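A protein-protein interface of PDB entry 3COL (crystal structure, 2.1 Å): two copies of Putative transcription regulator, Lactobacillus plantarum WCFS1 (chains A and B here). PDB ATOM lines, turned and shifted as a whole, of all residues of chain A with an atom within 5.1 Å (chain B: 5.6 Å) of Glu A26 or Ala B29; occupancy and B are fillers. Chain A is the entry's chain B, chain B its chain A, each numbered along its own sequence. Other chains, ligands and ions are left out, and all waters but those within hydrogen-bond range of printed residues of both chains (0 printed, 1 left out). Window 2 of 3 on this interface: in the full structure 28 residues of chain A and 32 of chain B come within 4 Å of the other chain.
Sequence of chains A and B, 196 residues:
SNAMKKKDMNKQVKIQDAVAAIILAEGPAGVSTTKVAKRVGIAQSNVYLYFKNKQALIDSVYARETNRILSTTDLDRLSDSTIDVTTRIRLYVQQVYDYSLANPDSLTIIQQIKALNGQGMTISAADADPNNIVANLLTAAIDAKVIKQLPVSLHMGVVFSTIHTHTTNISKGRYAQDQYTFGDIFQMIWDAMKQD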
ATOM      1  N   ALA A  21       9.495  26.111  30.081  1.00  0.00           N
ATOM      2  CA  ALA A  21      10.798  25.463  30.298  1.00  0.00           C
ATOM      3  C   ALA A  21      11.812  25.750  29.175  1.00  0.00           C
ATOM      4  O   ALA A  21      13.008  25.891  29.441  1.00  0.00           O
ATOM      5  CB  ALA A  21      10.639  23.958  30.517  1.00  0.00           C
ATOM      6  N   ILE A  22      11.333  25.862  27.935  1.00  0.00           N
ATOM      7  CA  ILE A  22      12.197  26.238  26.802  1.00  0.00           C
ATOM      8  C   ILE A  22      12.670  27.664  26.974  1.00  0.00           C
ATOM      9  O   ILE A  22      13.867  27.923  26.846  1.00  0.00           O
ATOM     10  CB  ILE A  22      11.524  26.125  25.386  1.00  0.00           C
ATOM     11  CG1 ILE A  22      11.283  24.679  24.992  1.00  0.00           C
ATOM     12  CG2 ILE A  22      12.413  26.796  24.293  1.00  0.00           C
ATOM     13  CD1 ILE A  22      10.360  24.542  23.777  1.00  0.00           C
ATOM     14  N   ILE A  23      11.732  28.578  27.241  1.00  0.00           N
ATOM     15  CA  ILE A  23      12.092  29.979  27.487  1.00  0.00           C
ATOM     16  C   ILE A  23      13.122  30.087  28.615  1.00  0.00           C
ATOM     17  O   ILE A  23      14.115  30.768  28.439  1.00  0.00           O
ATOM     18  CB  ILE A  23      10.872  30.894  27.719  1.00  0.00           C
ATOM     19  CG1 ILE A  23       9.981  30.900  26.463  1.00  0.00           C
ATOM     20  CG2 ILE A  23      11.319  32.334  28.043  1.00  0.00           C
ATOM     21  CD1 ILE A  23       8.452  31.103  26.757  1.00  0.00           C
ATOM     22  N   LEU A  24      12.905  29.390  29.737  1.00  0.00           N
ATOM     23  CA  LEU A  24      13.875  29.383  30.835  1.00  0.00           C
ATOM     24  C   LEU A  24      15.263  28.897  30.423  1.00  0.00           C
ATOM     25  O   LEU A  24      16.273  29.470  30.867  1.00  0.00           O
ATOM     26  CB  LEU A  24      13.380  28.522  31.990  1.00  0.00           C
ATOM     27  CG  LEU A  24      12.384  29.100  32.991  1.00  0.00           C
ATOM     28  CD1 LEU A  24      12.186  28.103  34.118  1.00  0.00           C
ATOM     29  CD2 LEU A  24      12.875  30.461  33.572  1.00  0.00           C
ATOM     30  N   ALA A  25      15.329  27.863  29.580  1.00  0.00           N
ATOM     31  CA  ALA A  25      16.612  27.230  29.267  1.00  0.00           C
ATOM     32  C   ALA A  25      17.314  27.857  28.062  1.00  0.00           C
ATOM     33  O   ALA A  25      18.534  27.971  28.047  1.00  0.00           O
ATOM     34  CB  ALA A  25      16.442  25.726  29.057  1.00  0.00           C
ATOM     35  N   GLU A  26      16.533  28.256  27.061  1.00  0.00           N
ATOM     36  CA  GLU A  26      17.063  28.658  25.759  1.00  0.00           C
ATOM     37  C   GLU A  26      16.557  30.031  25.323  1.00  0.00           C
ATOM     38  O   GLU A  26      16.996  30.550  24.304  1.00  0.00           O
ATOM     39  CB  GLU A  26      16.682  27.635  24.690  1.00  0.00           C
ATOM     40  CG  GLU A  26      17.335  26.269  24.830  1.00  0.00           C
ATOM     41  CD  GLU A  26      16.812  25.271  23.804  1.00  0.00           C
ATOM     42  OE1 GLU A  26      15.574  25.130  23.684  1.00  0.00           O
ATOM     43  OE2 GLU A  26      17.630  24.628  23.125  1.00  0.00           O
ATOM     44  N   GLY A  27      15.646  30.617  26.093  1.00  0.00           N
ATOM     45  CA  GLY A  27      15.076  31.928  25.751  1.00  0.00           C
ATOM     46  C   GLY A  27      13.922  31.854  24.745  1.00  0.00           C
ATOM     47  O   GLY A  27      13.709  30.803  24.132  1.00  0.00           O
ATOM     48  N   PRO A  28      13.190  32.990  24.568  1.00  0.00           N
ATOM     49  CA  PRO A  28      12.016  33.128  23.709  1.00  0.00           C
ATOM     50  C   PRO A  28      12.385  32.884  22.253  1.00  0.00           C
ATOM     51  O   PRO A  28      11.568  32.359  21.481  1.00  0.00           O
ATOM     52  CB  PRO A  28      11.593  34.607  23.873  1.00  0.00           C
ATOM     53  CG  PRO A  28      12.419  35.208  24.966  1.00  0.00           C
ATOM     54  CD  PRO A  28      13.558  34.267  25.233  1.00  0.00           C
ATOM     55  N   ALA A  29      13.609  33.277  21.878  1.00  0.00           N
ATOM     56  CA  ALA A  29      14.083  33.115  20.508  1.00  0.00           C
ATOM     57  C   ALA A  29      14.290  31.631  20.155  1.00  0.00           C
ATOM     58  O   ALA A  29      14.418  31.272  18.985  1.00  0.00           O
ATOM     59  CB  ALA A  29      15.367  33.934  20.284  1.00  0.00           C
ATOM     60  N   GLY A  30      14.326  30.786  21.186  1.00  0.00           N
ATOM     61  CA  GLY A  30      14.613  29.362  21.032  1.00  0.00           C
ATOM     62  C   GLY A  30      13.359  28.587  20.734  1.00  0.00           C
ATOM     63  O   GLY A  30      13.428  27.491  20.172  1.00  0.00           O
ATOM     64  N   LYS A  35      10.075  22.372  18.108  1.00  0.00           N
ATOM     65  CA  LYS A  35      10.654  21.989  19.385  1.00  0.00           C
ATOM     66  C   LYS A  35       9.566  21.814  20.451  1.00  0.00           C
ATOM     67  O   LYS A  35       9.633  20.897  21.281  1.00  0.00           O
ATOM     68  CB  LYS A  35      11.676  23.040  19.831  1.00  0.00           C
ATOM     69  CG  LYS A  35      12.301  22.810  21.214  1.00  0.00           C
ATOM     70  CD  LYS A  35      13.312  23.905  21.590  1.00  0.00           C
ATOM     71  CE  LYS A  35      14.677  23.640  20.920  1.00  0.00           C
ATOM     72  NZ  LYS A  35      15.274  22.363  21.419  1.00  0.00           N
ATOM     73  N   GLU B  26      18.041  34.064  17.304  1.00  0.00           N
ATOM     74  CA  GLU B  26      17.668  32.784  17.929  1.00  0.00           C
ATOM     75  C   GLU B  26      18.133  32.591  19.372  1.00  0.00           C
ATOM     76  O   GLU B  26      17.913  31.519  19.949  1.00  0.00           O
ATOM     77  CB  GLU B  26      18.129  31.594  17.096  1.00  0.00           C
ATOM     78  CG  GLU B  26      17.879  31.696  15.607  1.00  0.00           C
ATOM     79  CD  GLU B  26      18.581  30.579  14.860  1.00  0.00           C
ATOM     80  OE1 GLU B  26      19.279  30.858  13.854  1.00  0.00           O
ATOM     81  OE2 GLU B  26      18.452  29.414  15.299  1.00  0.00           O
ATOM     82  N   GLY B  27      18.741  33.620  19.962  1.00  0.00           N
ATOM     83  CA  GLY B  27      19.375  33.467  21.263  1.00  0.00           C
ATOM     84  C   GLY B  27      20.674  32.671  21.194  1.00  0.00           C
ATOM     85  O   GLY B  27      21.026  32.109  20.145  1.00  0.00           O
ATOM     86  N   PRO B  28      21.407  32.612  22.314  1.00  0.00           N
ATOM     87  CA  PRO B  28      22.699  31.943  22.339  1.00  0.00           C
ATOM     88  C   PRO B  28      22.618  30.456  21.982  1.00  0.00           C
ATOM     89  O   PRO B  28      23.511  29.933  21.351  1.00  0.00           O
ATOM     90  CB  PRO B  28      23.160  32.136  23.791  1.00  0.00           C
ATOM     91  CG  PRO B  28      22.401  33.265  24.283  1.00  0.00           C
ATOM     92  CD  PRO B  28      21.074  33.186  23.627  1.00  0.00           C
ATOM     93  N   ALA B  29      21.520  29.804  22.342  1.00  0.00           N
ATOM     94  CA  ALA B  29      21.294  28.401  21.987  1.00  0.00           C
ATOM     95  C   ALA B  29      21.290  28.157  20.466  1.00  0.00           C
ATOM     96  O   ALA B  29      21.601  27.059  20.015  1.00  0.00           O
ATOM     97  CB  ALA B  29      20.013  27.889  22.640  1.00  0.00           C
ATOM     98  N   GLY B  30      20.972  29.185  19.682  1.00  0.00           N
ATOM     99  CA  GLY B  30      20.959  29.053  18.231  1.00  0.00           C
ATOM    100  C   GLY B  30      22.343  29.055  17.587  1.00  0.00           C
ATOM    101  O   GLY B  30      22.475  28.707  16.425  1.00  0.00           O
ATOM    102  N   VAL B  31      23.377  29.457  18.321  1.00  0.00           N
ATOM    103  CA  VAL B  31      24.734  29.510  17.762  1.00  0.00           C
ATOM    104  C   VAL B  31      25.320  28.095  17.497  1.00  0.00           C
ATOM    105  O   VAL B  31      25.237  27.217  18.360  1.00  0.00           O
ATOM    106  CB  VAL B  31      25.682  30.343  18.673  1.00  0.00           C
ATOM    107  CG1 VAL B  31      27.136  30.301  18.186  1.00  0.00           C
ATOM    108  CG2 VAL B  31      25.197  31.816  18.784  1.00  0.00           C
ATOM    109  N   LYS B  54      31.253  26.077  19.923  1.00  0.00           N
ATOM    110  CA  LYS B  54      30.131  26.999  20.075  1.00  0.00           C
ATOM    111  C   LYS B  54      30.335  27.908  21.296  1.00  0.00           C
ATOM    112  O   LYS B  54      30.180  29.109  21.182  1.00  0.00           O
ATOM    113  CB  LYS B  54      28.809  26.208  20.164  1.00  0.00           C
ATOM    114  CG  LYS B  54      27.660  26.917  20.850  1.00  0.00           C
ATOM    115  CD  LYS B  54      26.467  25.966  21.093  1.00  0.00           C
ATOM    116  CE  LYS B  54      25.205  26.732  21.605  1.00  0.00           C
ATOM    117  NZ  LYS B  54      24.017  25.746  21.795  1.00  0.00           N
ATOM    118  N   ILE B  58      30.474  32.199  21.496  1.00  0.00           N
ATOM    119  CA  ILE B  58      29.624  32.999  22.395  1.00  0.00           C
ATOM    120  C   ILE B  58      30.494  33.857  23.355  1.00  0.00           C
ATOM    121  O   ILE B  58      30.235  35.065  23.542  1.00  0.00           O
ATOM    122  CB  ILE B  58      28.673  32.053  23.201  1.00  0.00           C
ATOM    123  CG1 ILE B  58      27.593  31.433  22.271  1.00  0.00           C
ATOM    124  CG2 ILE B  58      28.026  32.783  24.385  1.00  0.00           C
ATOM    125  CD1 ILE B  58      26.944  30.109  22.847  1.00  0.00           C
ATOM    126  N   LEU B 116      21.490  32.951  29.581  1.00  0.00           N
ATOM    127  CA  LEU B 116      21.756  31.538  29.268  1.00  0.00           C
ATOM    128  C   LEU B 116      22.834  30.886  30.155  1.00  0.00           C
ATOM    129  O   LEU B 116      22.788  29.667  30.419  1.00  0.00           O
ATOM    130  CB  LEU B 116      22.119  31.368  27.790  1.00  0.00           C
ATOM    131  CG  LEU B 116      22.091  29.935  27.266  1.00  0.00           C
ATOM    132  CD1 LEU B 116      20.813  29.694  26.465  1.00  0.00           C
ATOM    133  CD2 LEU B 116      23.340  29.626  26.428  1.00  0.00           C
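O of Ala B29 is in hydrogen-bond range of NZ of Lys B54 (3.3 Å).
The side-chain carboxylate (OE1) of Glu A26 is in salt-bridge range of the side-chain amino group (NZ) of Lys A35 (3.6 Å).
CD1 of Leu B116 touches O of Ala A25 (3.3 Å).
Glu A26 touches Ala B29 (CG to CB, 3.8 Å).
Leu B116 touches Glu A26.
Ala A29 touches Glu B26.
Ala A29 touches Gly B27 (CB to N, 3.4 Å).
Gly A30 touches Glu B26 (N to O, 3.9 Å).
Ile A22 touches none of the printed residues of chain B.
Ile A23 touches none of the printed residues of chain B.
Of the printed residues of chain B, Gly A30 touches Glu B26.
Printed residues of chain A within 4 Å of Gly B27: Ala A29 (3.4 Å).
Ala B29 touches just one residue of chain A: Glu A26.
Of the printed residues of chain A, Leu B116 touches Ala A25 and Glu A26.
The nearest residue of chain B that does not touch Glu A26 is Glu B26 (4.6 Å).
The nearest printed residue of chain A that does not touch Gly B27 is Glu A26 (4.8 Å).
Hydrophobic or aromatic side chains of chain B that line the printed part of chain A: Ala B29 and Leu B116.
Hydrophobic or aromatic side chains of chain A within 4 Å of the printed part of chain B: Ala A29.
Glu A26 touches Ala B29, and with the chains exchanged Ala A29 touches Glu B26.
Ala A29 touches Gly B27, but with the chains exchanged Gly A27 does not touch Ala B29 (6.2 Å).
Gly A30 touches Glu B26, but with the chains exchanged Glu A26 does not touch Gly B30 (6.2 Å).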
